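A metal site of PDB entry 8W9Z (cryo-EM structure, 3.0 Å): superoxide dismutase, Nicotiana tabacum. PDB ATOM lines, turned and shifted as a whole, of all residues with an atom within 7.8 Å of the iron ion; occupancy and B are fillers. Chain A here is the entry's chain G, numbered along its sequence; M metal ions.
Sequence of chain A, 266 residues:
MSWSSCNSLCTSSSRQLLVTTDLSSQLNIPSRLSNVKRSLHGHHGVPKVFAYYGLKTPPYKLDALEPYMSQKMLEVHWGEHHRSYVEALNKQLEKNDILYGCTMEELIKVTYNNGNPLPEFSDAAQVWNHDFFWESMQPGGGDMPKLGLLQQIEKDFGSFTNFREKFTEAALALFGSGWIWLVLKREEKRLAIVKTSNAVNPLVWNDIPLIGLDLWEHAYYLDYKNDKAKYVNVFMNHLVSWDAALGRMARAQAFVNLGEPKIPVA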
ATOM      1  N   HIS A  77      -0.833  24.453  15.448  1.00  0.00           N
ATOM      2  CA  HIS A  77       0.168  24.169  14.443  1.00  0.00           C
ATOM      3  C   HIS A  77       0.917  25.431  14.107  1.00  0.00           C
ATOM      4  O   HIS A  77       2.130  25.416  14.035  1.00  0.00           O
ATOM      5  CB  HIS A  77      -0.507  23.645  13.193  1.00  0.00           C
ATOM      6  CG  HIS A  77       0.404  22.909  12.266  1.00  0.00           C
ATOM      7  ND1 HIS A  77      -0.064  22.227  11.169  1.00  0.00           N
ATOM      8  CD2 HIS A  77       1.748  22.738  12.270  1.00  0.00           C
ATOM      9  CE1 HIS A  77       0.949  21.672  10.529  1.00  0.00           C
ATOM     10  NE2 HIS A  77       2.059  21.976  11.170  1.00  0.00           N
ATOM     11  N   TRP A  78       0.208  26.528  13.940  1.00  0.00           N
ATOM     12  CA  TRP A  78       0.884  27.738  13.498  1.00  0.00           C
ATOM     13  C   TRP A  78       1.487  28.426  14.668  1.00  0.00           C
ATOM     14  O   TRP A  78       2.653  28.787  14.657  1.00  0.00           O
ATOM     15  CB  TRP A  78      -0.120  28.662  12.832  1.00  0.00           C
ATOM     16  CG  TRP A  78       0.430  29.973  12.436  1.00  0.00           C
ATOM     17  CD1 TRP A  78       1.194  30.240  11.332  1.00  0.00           C
ATOM     18  CD2 TRP A  78       0.260  31.210  13.116  1.00  0.00           C
ATOM     19  NE1 TRP A  78       1.506  31.571  11.297  1.00  0.00           N
ATOM     20  CE2 TRP A  78       0.947  32.190  12.388  1.00  0.00           C
ATOM     21  CE3 TRP A  78      -0.412  31.583  14.281  1.00  0.00           C
ATOM     22  CZ2 TRP A  78       0.982  33.519  12.769  1.00  0.00           C
ATOM     23  CZ3 TRP A  78      -0.371  32.897  14.669  1.00  0.00           C
ATOM     24  CH2 TRP A  78       0.323  33.855  13.919  1.00  0.00           C
ATOM     25  N   HIS A  81       3.847  25.096  16.948  1.00  0.00           N
ATOM     26  CA  HIS A  81       4.824  24.336  16.218  1.00  0.00           C
ATOM     27  C   HIS A  81       5.637  25.200  15.307  1.00  0.00           C
ATOM     28  O   HIS A  81       6.859  25.098  15.290  1.00  0.00           O
ATOM     29  CB  HIS A  81       4.127  23.254  15.414  1.00  0.00           C
ATOM     30  CG  HIS A  81       3.554  22.158  16.246  1.00  0.00           C
ATOM     31  ND1 HIS A  81       4.323  21.102  16.698  1.00  0.00           N
ATOM     32  CD2 HIS A  81       2.300  21.938  16.691  1.00  0.00           C
ATOM     33  CE1 HIS A  81       3.549  20.287  17.404  1.00  0.00           C
ATOM     34  NE2 HIS A  81       2.325  20.774  17.409  1.00  0.00           N
ATOM     35  N   HIS A  82       4.993  26.105  14.587  1.00  0.00           N
ATOM     36  CA  HIS A  82       5.737  26.896  13.609  1.00  0.00           C
ATOM     37  C   HIS A  82       6.558  27.934  14.286  1.00  0.00           C
ATOM     38  O   HIS A  82       7.722  28.113  13.961  1.00  0.00           O
ATOM     39  CB  HIS A  82       4.770  27.539  12.629  1.00  0.00           C
ATOM     40  CG  HIS A  82       5.419  28.121  11.413  1.00  0.00           C
ATOM     41  ND1 HIS A  82       4.777  29.000  10.576  1.00  0.00           N
ATOM     42  CD2 HIS A  82       6.655  27.933  10.892  1.00  0.00           C
ATOM     43  CE1 HIS A  82       5.587  29.341   9.592  1.00  0.00           C
ATOM     44  NE2 HIS A  82       6.731  28.710   9.752  1.00  0.00           N
ATOM     45  N   TYR A  85       9.793  26.896  15.447  1.00  0.00           N
ATOM     46  CA  TYR A  85      10.811  26.616  14.478  1.00  0.00           C
ATOM     47  C   TYR A  85      11.503  27.910  14.157  1.00  0.00           C
ATOM     48  O   TYR A  85      12.725  27.957  14.140  1.00  0.00           O
ATOM     49  CB  TYR A  85      10.193  26.049  13.233  1.00  0.00           C
ATOM     50  CG  TYR A  85       9.916  24.581  13.292  1.00  0.00           C
ATOM     51  CD1 TYR A  85      10.927  23.673  13.537  1.00  0.00           C
ATOM     52  CD2 TYR A  85       8.644  24.079  13.088  1.00  0.00           C
ATOM     53  CE1 TYR A  85      10.693  22.318  13.586  1.00  0.00           C
ATOM     54  CE2 TYR A  85       8.388  22.722  13.136  1.00  0.00           C
ATOM     55  CZ  TYR A  85       9.423  21.847  13.388  1.00  0.00           C
ATOM     56  OH  TYR A  85       9.180  20.502  13.437  1.00  0.00           O
ATOM     57  N   GLN A 126      11.870  23.361   7.716  1.00  0.00           N
ATOM     58  CA  GLN A 126      10.532  23.330   8.244  1.00  0.00           C
ATOM     59  C   GLN A 126       9.861  24.660   8.096  1.00  0.00           C
ATOM     60  O   GLN A 126       8.674  24.715   7.810  1.00  0.00           O
ATOM     61  CB  GLN A 126      10.486  22.842   9.674  1.00  0.00           C
ATOM     62  CG  GLN A 126      10.625  21.339   9.801  1.00  0.00           C
ATOM     63  CD  GLN A 126       9.441  20.591   9.226  1.00  0.00           C
ATOM     64  OE1 GLN A 126       9.567  19.852   8.261  1.00  0.00           O
ATOM     65  NE2 GLN A 126       8.281  20.786   9.828  1.00  0.00           N
ATOM     66  N   ASN A 129       8.819  25.002   4.691  1.00  0.00           N
ATOM     67  CA  ASN A 129       7.804  24.028   4.386  1.00  0.00           C
ATOM     68  C   ASN A 129       6.486  24.482   4.909  1.00  0.00           C
ATOM     69  O   ASN A 129       5.494  24.450   4.212  1.00  0.00           O
ATOM     70  CB  ASN A 129       8.185  22.697   4.983  1.00  0.00           C
ATOM     71  CG  ASN A 129       9.171  21.938   4.130  1.00  0.00           C
ATOM     72  OD1 ASN A 129       9.404  22.303   2.991  1.00  0.00           O
ATOM     73  ND2 ASN A 129       9.742  20.887   4.688  1.00  0.00           N
ATOM     74  N   HIS A 130       6.467  24.942   6.144  1.00  0.00           N
ATOM     75  CA  HIS A 130       5.197  25.303   6.700  1.00  0.00           C
ATOM     76  C   HIS A 130       4.583  26.430   5.937  1.00  0.00           C
ATOM     77  O   HIS A 130       3.396  26.432   5.683  1.00  0.00           O
ATOM     78  CB  HIS A 130       5.299  25.621   8.168  1.00  0.00           C
ATOM     79  CG  HIS A 130       5.285  24.404   9.037  1.00  0.00           C
ATOM     80  ND1 HIS A 130       6.347  24.049   9.844  1.00  0.00           N
ATOM     81  CD2 HIS A 130       4.342  23.453   9.217  1.00  0.00           C
ATOM     82  CE1 HIS A 130       6.058  22.931  10.491  1.00  0.00           C
ATOM     83  NE2 HIS A 130       4.843  22.549  10.119  1.00  0.00           N
ATOM     84  N   PHE A 133       2.818  25.323   3.023  1.00  0.00           N
ATOM     85  CA  PHE A 133       1.603  24.609   3.333  1.00  0.00           C
ATOM     86  C   PHE A 133       0.449  25.526   3.607  1.00  0.00           C
ATOM     87  O   PHE A 133      -0.629  25.305   3.071  1.00  0.00           O
ATOM     88  CB  PHE A 133       1.853  23.757   4.557  1.00  0.00           C
ATOM     89  CG  PHE A 133       0.665  22.994   5.043  1.00  0.00           C
ATOM     90  CD1 PHE A 133       0.190  21.910   4.338  1.00  0.00           C
ATOM     91  CD2 PHE A 133       0.056  23.326   6.228  1.00  0.00           C
ATOM     92  CE1 PHE A 133      -0.903  21.192   4.797  1.00  0.00           C
ATOM     93  CE2 PHE A 133      -1.030  22.625   6.701  1.00  0.00           C
ATOM     94  CZ  PHE A 133      -1.506  21.552   5.977  1.00  0.00           C
ATOM     95  N   TRP A 134       0.641  26.575   4.373  1.00  0.00           N
ATOM     96  CA  TRP A 134      -0.508  27.381   4.723  1.00  0.00           C
ATOM     97  C   TRP A 134      -1.049  27.923   3.455  1.00  0.00           C
ATOM     98  O   TRP A 134      -2.245  27.980   3.267  1.00  0.00           O
ATOM     99  CB  TRP A 134      -0.152  28.515   5.650  1.00  0.00           C
ATOM    100  CG  TRP A 134       0.567  28.142   6.869  1.00  0.00           C
ATOM    101  CD1 TRP A 134       1.806  28.566   7.252  1.00  0.00           C
ATOM    102  CD2 TRP A 134       0.105  27.274   7.907  1.00  0.00           C
ATOM    103  NE1 TRP A 134       2.143  27.999   8.450  1.00  0.00           N
ATOM    104  CE2 TRP A 134       1.119  27.204   8.874  1.00  0.00           C
ATOM    105  CE3 TRP A 134      -1.065  26.546   8.104  1.00  0.00           C
ATOM    106  CZ2 TRP A 134       0.998  26.441  10.024  1.00  0.00           C
ATOM    107  CZ3 TRP A 134      -1.191  25.789   9.243  1.00  0.00           C
ATOM    108  CH2 TRP A 134      -0.165  25.742  10.191  1.00  0.00           C
ATOM    109  N   GLY A 178       6.445  13.241   7.530  1.00  0.00           N
ATOM    110  CA  GLY A 178       6.986  13.625   6.242  1.00  0.00           C
ATOM    111  C   GLY A 178       6.055  14.529   5.500  1.00  0.00           C
ATOM    112  O   GLY A 178       5.086  14.984   6.077  1.00  0.00           O
ATOM    113  N   TRP A 179       6.348  14.816   4.242  1.00  0.00           N
ATOM    114  CA  TRP A 179       5.456  15.633   3.456  1.00  0.00           C
ATOM    115  C   TRP A 179       5.255  15.019   2.092  1.00  0.00           C
ATOM    116  O   TRP A 179       6.105  14.278   1.639  1.00  0.00           O
ATOM    117  CB  TRP A 179       6.041  17.025   3.292  1.00  0.00           C
ATOM    118  CG  TRP A 179       6.335  17.802   4.522  1.00  0.00           C
ATOM    119  CD1 TRP A 179       7.331  17.582   5.427  1.00  0.00           C
ATOM    120  CD2 TRP A 179       5.669  18.994   4.957  1.00  0.00           C
ATOM    121  NE1 TRP A 179       7.304  18.525   6.412  1.00  0.00           N
ATOM    122  CE2 TRP A 179       6.286  19.407   6.149  1.00  0.00           C
ATOM    123  CE3 TRP A 179       4.595  19.735   4.465  1.00  0.00           C
ATOM    124  CZ2 TRP A 179       5.870  20.531   6.850  1.00  0.00           C
ATOM    125  CZ3 TRP A 179       4.193  20.844   5.153  1.00  0.00           C
ATOM    126  CH2 TRP A 179       4.823  21.230   6.334  1.00  0.00           C
ATOM    127  N   LEU A 213       1.404  18.713   1.402  1.00  0.00           N
ATOM    128  CA  LEU A 213       0.601  18.342   2.563  1.00  0.00           C
ATOM    129  C   LEU A 213       1.492  17.899   3.688  1.00  0.00           C
ATOM    130  O   LEU A 213       2.504  17.265   3.461  1.00  0.00           O
ATOM    131  CB  LEU A 213      -0.338  17.221   2.184  1.00  0.00           C
ATOM    132  CG  LEU A 213      -1.235  16.589   3.243  1.00  0.00           C
ATOM    133  CD1 LEU A 213      -2.081  17.650   3.927  1.00  0.00           C
ATOM    134  CD2 LEU A 213      -2.112  15.533   2.590  1.00  0.00           C
ATOM    135  N   ASP A 214       1.100  18.212   4.923  1.00  0.00           N
ATOM    136  CA  ASP A 214       1.916  17.861   6.077  1.00  0.00           C
ATOM    137  C   ASP A 214       1.400  16.571   6.606  1.00  0.00           C
ATOM    138  O   ASP A 214       0.285  16.496   7.082  1.00  0.00           O
ATOM    139  CB  ASP A 214       1.767  18.922   7.160  1.00  0.00           C
ATOM    140  CG  ASP A 214       2.821  18.813   8.225  1.00  0.00           C
ATOM    141  OD1 ASP A 214       3.652  17.899   8.144  1.00  0.00           O
ATOM    142  OD2 ASP A 214       2.847  19.665   9.132  1.00  0.00           O
ATOM    143  N   LEU A 215       2.214  15.541   6.523  1.00  0.00           N
ATOM    144  CA  LEU A 215       1.791  14.259   6.989  1.00  0.00           C
ATOM    145  C   LEU A 215       2.283  14.025   8.378  1.00  0.00           C
ATOM    146  O   LEU A 215       2.045  12.983   8.957  1.00  0.00           O
ATOM    147  CB  LEU A 215       2.271  13.171   6.049  1.00  0.00           C
ATOM    148  CG  LEU A 215       1.559  13.206   4.695  1.00  0.00           C
ATOM    149  CD1 LEU A 215       2.085  12.110   3.798  1.00  0.00           C
ATOM    150  CD2 LEU A 215       0.064  13.052   4.903  1.00  0.00           C
ATOM    151  N   TRP A 216       2.969  15.011   8.941  1.00  0.00           N
ATOM    152  CA  TRP A 216       3.385  14.882  10.314  1.00  0.00           C
ATOM    153  C   TRP A 216       2.127  14.813  11.129  1.00  0.00           C
ATOM    154  O   TRP A 216       1.158  15.499  10.836  1.00  0.00           O
ATOM    155  CB  TRP A 216       4.185  16.090  10.764  1.00  0.00           C
ATOM    156  CG  TRP A 216       5.585  16.134  10.327  1.00  0.00           C
ATOM    157  CD1 TRP A 216       6.057  16.040   9.060  1.00  0.00           C
ATOM    158  CD2 TRP A 216       6.731  16.304  11.173  1.00  0.00           C
ATOM    159  NE1 TRP A 216       7.414  16.131   9.049  1.00  0.00           N
ATOM    160  CE2 TRP A 216       7.856  16.295  10.332  1.00  0.00           C
ATOM    161  CE3 TRP A 216       6.907  16.446  12.535  1.00  0.00           C
ATOM    162  CZ2 TRP A 216       9.144  16.427  10.834  1.00  0.00           C
ATOM    163  CZ3 TRP A 216       8.176  16.581  13.028  1.00  0.00           C
ATOM    164  CH2 TRP A 216       9.283  16.575  12.180  1.00  0.00           C
ATOM    165  N   GLU A 217       2.134  14.017  12.173  1.00  0.00           N
ATOM    166  CA  GLU A 217       0.945  13.838  12.969  1.00  0.00           C
ATOM    167  C   GLU A 217       0.460  15.065  13.659  1.00  0.00           C
ATOM    168  O   GLU A 217      -0.717  15.184  13.940  1.00  0.00           O
ATOM    169  CB  GLU A 217       1.146  12.728  13.988  1.00  0.00           C
ATOM    170  CG  GLU A 217       1.435  11.373  13.376  1.00  0.00           C
ATOM    171  CD  GLU A 217       1.633  10.289  14.409  1.00  0.00           C
ATOM    172  OE1 GLU A 217       1.826  10.634  15.596  1.00  0.00           O
ATOM    173  OE2 GLU A 217       1.621   9.101  14.047  1.00  0.00           O
ATOM    174  N   HIS A 218       1.341  16.023  13.910  1.00  0.00           N
ATOM    175  CA  HIS A 218       0.923  17.168  14.675  1.00  0.00           C
ATOM    176  C   HIS A 218      -0.215  17.817  13.967  1.00  0.00           C
ATOM    177  O   HIS A 218      -1.099  18.389  14.594  1.00  0.00           O
ATOM    178  CB  HIS A 218       2.053  18.155  14.996  1.00  0.00           C
ATOM    179  CG  HIS A 218       2.857  18.609  13.808  1.00  0.00           C
ATOM    180  ND1 HIS A 218       4.228  18.536  13.783  1.00  0.00           N
ATOM    181  CD2 HIS A 218       2.487  19.190  12.640  1.00  0.00           C
ATOM    182  CE1 HIS A 218       4.670  19.036  12.641  1.00  0.00           C
ATOM    183  NE2 HIS A 218       3.636  19.429  11.935  1.00  0.00           N
ATOM    184  N   ALA A 219      -0.195  17.751  12.662  1.00  0.00           N
ATOM    185  CA  ALA A 219      -1.257  18.351  11.888  1.00  0.00           C
ATOM    186  C   ALA A 219      -2.621  17.749  12.098  1.00  0.00           C
ATOM    187  O   ALA A 219      -3.585  18.489  12.224  1.00  0.00           O
ATOM    188  CB  ALA A 219      -0.906  18.297  10.430  1.00  0.00           C
HETATM  189 FE    FE M   1       3.635  20.947  10.461  1.00  0.00          FE
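A ring nitrogen (ND1) of His 130 sits at hydrogen-bond distance from the backbone carbonyl oxygen (O) of Gln 126, 3.2 Å away.
The backbone NH of Trp 216 is in hydrogen-bond range of the side-chain carboxylate of Asp 214.
The indole nitrogen (NE1) of Trp 134 sits close to the backbone carbonyl oxygen (O) of His 130 (3.4 Å).
The backbone carbonyl oxygen of His 77 sits at hydrogen-bond distance from the backbone NH of His 82 (3.0 Å).
The iron ion is bound by the side-chain carboxylate (OD2) of Asp 214 (2.0 Å), a ring nitrogen (NE2) of His 77 (2.0 Å), a ring nitrogen (NE2) of His 130 (2.0 Å) and a ring nitrogen (NE2) of His 218 (2.1 Å).
The iron ion has four donor atoms within binding distance.
Of the 19 residues printed, 4 come within 4 Å of the iron ion.
The nearest printed residue that does not touch the iron ion is Trp 179 (4.3 Å).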
